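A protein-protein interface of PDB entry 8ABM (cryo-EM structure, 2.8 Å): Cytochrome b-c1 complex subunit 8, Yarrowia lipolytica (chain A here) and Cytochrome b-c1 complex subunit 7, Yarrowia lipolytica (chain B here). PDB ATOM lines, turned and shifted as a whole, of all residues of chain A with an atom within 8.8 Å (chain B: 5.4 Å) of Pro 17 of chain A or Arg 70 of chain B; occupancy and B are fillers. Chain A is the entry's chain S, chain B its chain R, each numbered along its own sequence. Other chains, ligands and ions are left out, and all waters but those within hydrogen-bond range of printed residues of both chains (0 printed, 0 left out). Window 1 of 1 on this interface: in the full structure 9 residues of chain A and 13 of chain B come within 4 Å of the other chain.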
ATOM      1  N   MET A  14     -16.989 -14.243  36.183  1.00  0.00           N
ATOM      2  CA  MET A  14     -15.678 -14.806  35.910  1.00  0.00           C
ATOM      3  C   MET A  14     -15.308 -14.613  34.440  1.00  0.00           C
ATOM      4  O   MET A  14     -14.129 -14.518  34.119  1.00  0.00           O
ATOM      5  CB  MET A  14     -15.641 -16.298  36.245  1.00  0.00           C
ATOM      6  CG  MET A  14     -14.242 -16.858  36.399  1.00  0.00           C
ATOM      7  SD  MET A  14     -13.456 -16.214  37.888  1.00  0.00           S
ATOM      8  CE  MET A  14     -14.557 -16.917  39.114  1.00  0.00           C
ATOM      9  N   GLY A  15     -16.304 -14.533  33.556  1.00  0.00           N
ATOM     10  CA  GLY A  15     -16.024 -14.291  32.152  1.00  0.00           C
ATOM     11  C   GLY A  15     -16.211 -15.548  31.306  1.00  0.00           C
ATOM     12  O   GLY A  15     -15.783 -15.596  30.152  1.00  0.00           O
ATOM     13  N   SER A  16     -16.870 -16.553  31.896  1.00  0.00           N
ATOM     14  CA  SER A  16     -17.352 -17.726  31.188  1.00  0.00           C
ATOM     15  C   SER A  16     -18.376 -17.304  30.136  1.00  0.00           C
ATOM     16  O   SER A  16     -19.154 -16.375  30.364  1.00  0.00           O
ATOM     17  CB  SER A  16     -17.947 -18.705  32.168  1.00  0.00           C
ATOM     18  OG  SER A  16     -18.552 -19.804  31.503  1.00  0.00           O
ATOM     19  N   PRO A  17     -18.430 -17.976  28.964  1.00  0.00           N
ATOM     20  CA  PRO A  17     -19.597 -17.871  28.090  1.00  0.00           C
ATOM     21  C   PRO A  17     -20.777 -18.350  28.928  1.00  0.00           C
ATOM     22  O   PRO A  17     -20.574 -19.105  29.875  1.00  0.00           O
ATOM     23  CB  PRO A  17     -19.321 -18.922  27.015  1.00  0.00           C
ATOM     24  CG  PRO A  17     -17.822 -19.045  26.998  1.00  0.00           C
ATOM     25  CD  PRO A  17     -17.389 -18.863  28.432  1.00  0.00           C
ATOM     26  N   PRO A  18     -22.026 -17.912  28.661  1.00  0.00           N
ATOM     27  CA  PRO A  18     -23.160 -18.311  29.499  1.00  0.00           C
ATOM     28  C   PRO A  18     -23.296 -19.829  29.530  1.00  0.00           C
ATOM     29  O   PRO A  18     -23.150 -20.498  28.509  1.00  0.00           O
ATOM     30  CB  PRO A  18     -24.349 -17.667  28.788  1.00  0.00           C
ATOM     31  CG  PRO A  18     -23.726 -16.484  28.080  1.00  0.00           C
ATOM     32  CD  PRO A  18     -22.408 -17.012  27.562  1.00  0.00           C
ATOM     33  N   GLN A  19     -23.467 -20.361  30.733  1.00  0.00           N
ATOM     34  CA  GLN A  19     -23.627 -21.792  30.894  1.00  0.00           C
ATOM     35  C   GLN A  19     -25.102 -22.078  31.087  1.00  0.00           C
ATOM     36  O   GLN A  19     -25.800 -21.332  31.765  1.00  0.00           O
ATOM     37  CB  GLN A  19     -22.850 -22.278  32.107  1.00  0.00           C
ATOM     38  CG  GLN A  19     -21.437 -21.745  32.106  1.00  0.00           C
ATOM     39  CD  GLN A  19     -20.550 -22.515  33.048  1.00  0.00           C
ATOM     40  OE1 GLN A  19     -20.981 -23.450  33.729  1.00  0.00           O
ATOM     41  NE2 GLN A  19     -19.289 -22.112  33.099  1.00  0.00           N
ATOM     42  N   LYS A  20     -25.564 -23.139  30.444  1.00  0.00           N
ATOM     43  CA  LYS A  20     -26.930 -23.571  30.610  1.00  0.00           C
ATOM     44  C   LYS A  20     -26.929 -25.054  30.293  1.00  0.00           C
ATOM     45  O   LYS A  20     -26.208 -25.488  29.408  1.00  0.00           O
ATOM     46  CB  LYS A  20     -27.828 -22.775  29.665  1.00  0.00           C
ATOM     47  CG  LYS A  20     -29.304 -23.103  29.795  1.00  0.00           C
ATOM     48  CD  LYS A  20     -30.207 -22.087  29.163  1.00  0.00           C
ATOM     49  CE  LYS A  20     -31.667 -22.453  29.326  1.00  0.00           C
ATOM     50  NZ  LYS A  20     -32.531 -21.631  28.445  1.00  0.00           N
ATOM     51  N   ILE A  22     -26.003 -27.731  32.063  1.00  0.00           N
ATOM     52  CA  ILE A  22     -25.130 -28.677  32.733  1.00  0.00           C
ATOM     53  C   ILE A  22     -25.549 -28.825  34.190  1.00  0.00           C
ATOM     54  O   ILE A  22     -25.609 -27.838  34.918  1.00  0.00           O
ATOM     55  CB  ILE A  22     -23.671 -28.214  32.637  1.00  0.00           C
ATOM     56  CG1 ILE A  22     -23.272 -27.898  31.194  1.00  0.00           C
ATOM     57  CG2 ILE A  22     -22.753 -29.229  33.303  1.00  0.00           C
ATOM     58  CD1 ILE A  22     -21.999 -27.073  31.083  1.00  0.00           C
ATOM     59  N   ASP B  46     -11.728 -26.290  19.915  1.00  0.00           N
ATOM     60  CA  ASP B  46     -11.757 -25.993  21.338  1.00  0.00           C
ATOM     61  C   ASP B  46     -10.364 -25.650  21.859  1.00  0.00           C
ATOM     62  O   ASP B  46     -10.239 -25.036  22.913  1.00  0.00           O
ATOM     63  CB  ASP B  46     -12.305 -27.158  22.155  1.00  0.00           C
ATOM     64  CG  ASP B  46     -13.703 -27.603  21.758  1.00  0.00           C
ATOM     65  OD1 ASP B  46     -14.509 -26.737  21.356  1.00  0.00           O
ATOM     66  OD2 ASP B  46     -13.982 -28.823  21.855  1.00  0.00           O
ATOM     67  N   GLU B  50      -7.937 -18.266  23.173  1.00  0.00           N
ATOM     68  CA  GLU B  50      -9.079 -17.380  23.054  1.00  0.00           C
ATOM     69  C   GLU B  50      -8.858 -16.040  23.748  1.00  0.00           C
ATOM     70  O   GLU B  50      -9.731 -15.177  23.673  1.00  0.00           O
ATOM     71  CB  GLU B  50     -10.305 -18.059  23.642  1.00  0.00           C
ATOM     72  CG  GLU B  50     -10.199 -18.096  25.155  1.00  0.00           C
ATOM     73  CD  GLU B  50     -11.495 -18.385  25.890  1.00  0.00           C
ATOM     74  OE1 GLU B  50     -12.047 -17.433  26.495  1.00  0.00           O
ATOM     75  OE2 GLU B  50     -11.958 -19.554  25.862  1.00  0.00           O
ATOM     76  N   LEU B  59     -16.021 -15.666  19.616  1.00  0.00           N
ATOM     77  CA  LEU B  59     -16.764 -16.551  20.494  1.00  0.00           C
ATOM     78  C   LEU B  59     -18.144 -15.988  20.802  1.00  0.00           C
ATOM     79  O   LEU B  59     -19.101 -16.748  20.936  1.00  0.00           O
ATOM     80  CB  LEU B  59     -15.962 -16.829  21.762  1.00  0.00           C
ATOM     81  CG  LEU B  59     -14.816 -17.817  21.559  1.00  0.00           C
ATOM     82  CD1 LEU B  59     -13.885 -17.822  22.753  1.00  0.00           C
ATOM     83  CD2 LEU B  59     -15.326 -19.215  21.251  1.00  0.00           C
ATOM     84  N   LEU B  62     -20.711 -16.960  18.172  1.00  0.00           N
ATOM     85  CA  LEU B  62     -21.191 -18.326  18.035  1.00  0.00           C
ATOM     86  C   LEU B  62     -22.692 -18.389  18.283  1.00  0.00           C
ATOM     87  O   LEU B  62     -23.203 -17.700  19.168  1.00  0.00           O
ATOM     88  CB  LEU B  62     -20.509 -19.194  19.081  1.00  0.00           C
ATOM     89  CG  LEU B  62     -19.143 -19.737  18.699  1.00  0.00           C
ATOM     90  CD1 LEU B  62     -18.672 -20.663  19.805  1.00  0.00           C
ATOM     91  CD2 LEU B  62     -19.228 -20.480  17.372  1.00  0.00           C
ATOM     92  N   THR B  65     -26.525 -22.421  20.933  1.00  0.00           N
ATOM     93  CA  THR B  65     -26.388 -23.863  21.005  1.00  0.00           C
ATOM     94  C   THR B  65     -24.923 -24.291  20.953  1.00  0.00           C
ATOM     95  O   THR B  65     -24.483 -25.067  21.793  1.00  0.00           O
ATOM     96  CB  THR B  65     -27.110 -24.489  19.808  1.00  0.00           C
ATOM     97  OG1 THR B  65     -28.467 -24.046  19.866  1.00  0.00           O
ATOM     98  CG2 THR B  65     -27.041 -25.998  19.733  1.00  0.00           C
ATOM     99  N   GLU B  66     -24.199 -23.831  19.924  1.00  0.00           N
ATOM    100  CA  GLU B  66     -22.795 -24.172  19.746  1.00  0.00           C
ATOM    101  C   GLU B  66     -22.006 -23.688  20.953  1.00  0.00           C
ATOM    102  O   GLU B  66     -21.064 -24.338  21.397  1.00  0.00           O
ATOM    103  CB  GLU B  66     -22.207 -23.536  18.483  1.00  0.00           C
ATOM    104  CG  GLU B  66     -22.726 -24.142  17.197  1.00  0.00           C
ATOM    105  CD  GLU B  66     -21.933 -25.304  16.614  1.00  0.00           C
ATOM    106  OE1 GLU B  66     -21.913 -25.432  15.371  1.00  0.00           O
ATOM    107  OE2 GLU B  66     -21.352 -26.092  17.396  1.00  0.00           O
ATOM    108  N   SER B  67     -22.406 -22.535  21.478  1.00  0.00           N
ATOM    109  CA  SER B  67     -21.672 -21.977  22.584  1.00  0.00           C
ATOM    110  C   SER B  67     -21.879 -22.816  23.836  1.00  0.00           C
ATOM    111  O   SER B  67     -20.921 -23.031  24.571  1.00  0.00           O
ATOM    112  CB  SER B  67     -22.051 -20.568  22.813  1.00  0.00           C
ATOM    113  OG  SER B  67     -21.205 -20.001  23.801  1.00  0.00           O
ATOM    114  N   TYR B  68     -23.128 -23.251  24.067  1.00  0.00           N
ATOM    115  CA  TYR B  68     -23.442 -24.029  25.251  1.00  0.00           C
ATOM    116  C   TYR B  68     -22.705 -25.348  25.180  1.00  0.00           C
ATOM    117  O   TYR B  68     -22.254 -25.824  26.209  1.00  0.00           O
ATOM    118  CB  TYR B  68     -24.931 -24.332  25.421  1.00  0.00           C
ATOM    119  CG  TYR B  68     -25.750 -23.117  25.752  1.00  0.00           C
ATOM    120  CD1 TYR B  68     -25.328 -22.196  26.701  1.00  0.00           C
ATOM    121  CD2 TYR B  68     -26.938 -22.868  25.090  1.00  0.00           C
ATOM    122  CE1 TYR B  68     -26.065 -21.056  26.981  1.00  0.00           C
ATOM    123  CE2 TYR B  68     -27.692 -21.740  25.366  1.00  0.00           C
ATOM    124  CZ  TYR B  68     -27.252 -20.827  26.310  1.00  0.00           C
ATOM    125  OH  TYR B  68     -28.001 -19.715  26.575  1.00  0.00           O
ATOM    126  N   ASP B  69     -22.595 -25.903  23.970  1.00  0.00           N
ATOM    127  CA  ASP B  69     -21.961 -27.195  23.823  1.00  0.00           C
ATOM    128  C   ASP B  69     -20.465 -27.075  24.079  1.00  0.00           C
ATOM    129  O   ASP B  69     -19.842 -28.008  24.586  1.00  0.00           O
ATOM    130  CB  ASP B  69     -22.188 -27.770  22.434  1.00  0.00           C
ATOM    131  CG  ASP B  69     -23.616 -28.233  22.193  1.00  0.00           C
ATOM    132  OD1 ASP B  69     -24.425 -28.214  23.147  1.00  0.00           O
ATOM    133  OD2 ASP B  69     -23.917 -28.613  21.038  1.00  0.00           O
ATOM    134  N   ARG B  70     -19.887 -25.953  23.650  1.00  0.00           N
ATOM    135  CA  ARG B  70     -18.467 -25.750  23.836  1.00  0.00           C
ATOM    136  C   ARG B  70     -18.175 -25.683  25.333  1.00  0.00           C
ATOM    137  O   ARG B  70     -17.221 -26.295  25.805  1.00  0.00           O
ATOM    138  CB  ARG B  70     -18.021 -24.510  23.059  1.00  0.00           C
ATOM    139  CG  ARG B  70     -16.614 -24.038  23.391  1.00  0.00           C
ATOM    140  CD  ARG B  70     -16.147 -22.877  22.545  1.00  0.00           C
ATOM    141  NE  ARG B  70     -14.837 -22.395  22.966  1.00  0.00           N
ATOM    142  CZ  ARG B  70     -14.649 -21.537  23.967  1.00  0.00           C
ATOM    143  NH1 ARG B  70     -13.424 -21.152  24.285  1.00  0.00           N
ATOM    144  NH2 ARG B  70     -15.686 -21.074  24.650  1.00  0.00           N
ATOM    145  N   VAL B  71     -19.022 -24.961  26.073  1.00  0.00           N
ATOM    146  CA  VAL B  71     -18.804 -24.820  27.499  1.00  0.00           C
ATOM    147  C   VAL B  71     -18.838 -26.200  28.130  1.00  0.00           C
ATOM    148  O   VAL B  71     -17.980 -26.531  28.938  1.00  0.00           O
ATOM    149  CB  VAL B  71     -19.820 -23.883  28.165  1.00  0.00           C
ATOM    150  CG1 VAL B  71     -19.954 -24.165  29.650  1.00  0.00           C
ATOM    151  CG2 VAL B  71     -19.413 -22.440  27.956  1.00  0.00           C
ATOM    152  N   TYR B  72     -19.782 -27.029  27.710  1.00  0.00           N
ATOM    153  CA  TYR B  72     -19.804 -28.363  28.268  1.00  0.00           C
ATOM    154  C   TYR B  72     -18.540 -29.153  27.931  1.00  0.00           C
ATOM    155  O   TYR B  72     -17.984 -29.797  28.806  1.00  0.00           O
ATOM    156  CB  TYR B  72     -21.060 -29.104  27.842  1.00  0.00           C
ATOM    157  CG  TYR B  72     -21.027 -30.531  28.293  1.00  0.00           C
ATOM    158  CD1 TYR B  72     -21.013 -30.850  29.645  1.00  0.00           C
ATOM    159  CD2 TYR B  72     -20.967 -31.562  27.370  1.00  0.00           C
ATOM    160  CE1 TYR B  72     -20.950 -32.167  30.070  1.00  0.00           C
ATOM    161  CE2 TYR B  72     -20.946 -32.887  27.781  1.00  0.00           C
ATOM    162  CZ  TYR B  72     -20.930 -33.189  29.134  1.00  0.00           C
ATOM    163  OH  TYR B  72     -20.883 -34.489  29.560  1.00  0.00           O
ATOM    164  N   ARG B  73     -18.087 -29.135  26.680  1.00  0.00           N
ATOM    165  CA  ARG B  73     -16.879 -29.879  26.356  1.00  0.00           C
ATOM    166  C   ARG B  73     -15.689 -29.392  27.176  1.00  0.00           C
ATOM    167  O   ARG B  73     -14.863 -30.213  27.549  1.00  0.00           O
ATOM    168  CB  ARG B  73     -16.520 -29.796  24.876  1.00  0.00           C
ATOM    169  CG  ARG B  73     -17.429 -30.627  23.990  1.00  0.00           C
ATOM    170  CD  ARG B  73     -16.966 -30.711  22.546  1.00  0.00           C
ATOM    171  NE  ARG B  73     -16.660 -29.407  21.979  1.00  0.00           N
ATOM    172  CZ  ARG B  73     -17.539 -28.570  21.448  1.00  0.00           C
ATOM    173  NH1 ARG B  73     -17.113 -27.406  21.003  1.00  0.00           N
ATOM    174  NH2 ARG B  73     -18.823 -28.887  21.367  1.00  0.00           N
ATOM    175  N   LEU B  74     -15.582 -28.081  27.432  1.00  0.00           N
ATOM    176  CA  LEU B  74     -14.430 -27.619  28.193  1.00  0.00           C
ATOM    177  C   LEU B  74     -14.522 -28.113  29.627  1.00  0.00           C
ATOM    178  O   LEU B  74     -13.507 -28.502  30.195  1.00  0.00           O
ATOM    179  CB  LEU B  74     -14.299 -26.099  28.173  1.00  0.00           C
ATOM    180  CG  LEU B  74     -14.083 -25.489  26.793  1.00  0.00           C
ATOM    181  CD1 LEU B  74     -13.968 -23.974  26.880  1.00  0.00           C
ATOM    182  CD2 LEU B  74     -12.876 -26.100  26.093  1.00  0.00           C
ATOM    183  N   ILE B  75     -15.735 -28.127  30.179  1.00  0.00           N
ATOM    184  CA  ILE B  75     -15.872 -28.499  31.569  1.00  0.00           C
ATOM    185  C   ILE B  75     -15.618 -29.986  31.706  1.00  0.00           C
ATOM    186  O   ILE B  75     -14.898 -30.404  32.599  1.00  0.00           O
ATOM    187  CB  ILE B  75     -17.246 -28.099  32.095  1.00  0.00           C
ATOM    188  CG1 ILE B  75     -17.222 -26.612  32.429  1.00  0.00           C
ATOM    189  CG2 ILE B  75     -17.652 -28.951  33.286  1.00  0.00           C
ATOM    190  CD1 ILE B  75     -18.599 -26.031  32.597  1.00  0.00           C
ATOM    191  N   TYR B 101     -16.289 -25.616  13.949  1.00  0.00           N
ATOM    192  CA  TYR B 101     -17.466 -24.806  14.206  1.00  0.00           C
ATOM    193  C   TYR B 101     -17.035 -23.348  14.335  1.00  0.00           C
ATOM    194  O   TYR B 101     -17.829 -22.451  14.105  1.00  0.00           O
ATOM    195  CB  TYR B 101     -18.223 -25.310  15.444  1.00  0.00           C
ATOM    196  CG  TYR B 101     -17.413 -25.155  16.703  1.00  0.00           C
ATOM    197  CD1 TYR B 101     -17.443 -23.966  17.420  1.00  0.00           C
ATOM    198  CD2 TYR B 101     -16.542 -26.154  17.122  1.00  0.00           C
ATOM    199  CE1 TYR B 101     -16.647 -23.785  18.545  1.00  0.00           C
ATOM    200  CE2 TYR B 101     -15.733 -25.981  18.238  1.00  0.00           C
ATOM    201  CZ  TYR B 101     -15.790 -24.796  18.962  1.00  0.00           C
ATOM    202  OH  TYR B 101     -14.980 -24.610  20.052  1.00  0.00           O
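The guanidinium group of Arg 70 of chain B lies within salt-bridge range of the side-chain carboxylate of Glu 50 of chain B (2.7 Å). OG of Ser 16 of chain A lies within hydrogen-bond range of NE2 of Gln 19 of chain A, at 2.9 Å.
Pro 17 of chain A touches Ser 67 of chain B. Arg 70 of chain B touches Pro 17 of chain A (NH2 to CG, 3.8 Å). Val 71 of chain B touches Pro 17 of chain A (CG2 to CB, 3.6 Å). Pro 18 of chain A touches Tyr 68 of chain B. Gln 19 of chain A touches Val 71 of chain B. OE1 of Gln 19 of chain A touches CD1 of Ile 75 of chain B, at 3.7 Å. Lys 20 of chain A touches Tyr 68 of chain B (CB to CE1, 3.6 Å). CG1 of Val 71 of chain B touches CD1 of Ile 22 of chain A (3.8 Å). Ile 22 of chain A touches Tyr 72 of chain B. CD1 of Ile 75 of chain B touches CD1 of Ile 22 of chain A, 3.9 Å away.
Of chain B, only Ser 67, Arg 70 and Val 71 come within 4 Å of Pro 17 of chain A. Of the printed residues of chain B, Lys 20 of chain A touches Tyr 68 (3.6 Å). Of the printed residues of chain B, Ile 22 of chain A touches Val 71, Tyr 72 and Ile 75. Of the printed residues of chain A, Tyr 68 of chain B touches Pro 18 and Lys 20. Of the printed residues of chain A, Val 71 of chain B touches Pro 17 (3.6 Å), Gln 19 (3.8 Å) and Ile 22 (3.8 Å). Of the printed residues of chain A, Tyr 72 of chain B touches Ile 22. The nearest printed residue of chain B that does not touch Pro 17 of chain A is Glu 50 of chain B (5.9 Å). The nearest printed residue of chain B that does not touch Lys 20 of chain A is Val 71 of chain B (5.8 Å).
Of the 16 printed residues of chain B, 6 touch a printed residue of chain A. Of the 8 printed residues of chain A, 5 touch a printed residue of chain B. Printed residues of chain A that touch a printed residue of chain B: Pro 17, Pro 18, Gln 19, Lys 20 and Ile 22. Hydrophobic or aromatic side chains of chain A that line the printed part of chain B: Pro 17 and Ile 22. Among the printed residues, 10 pairs touch across the chains.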
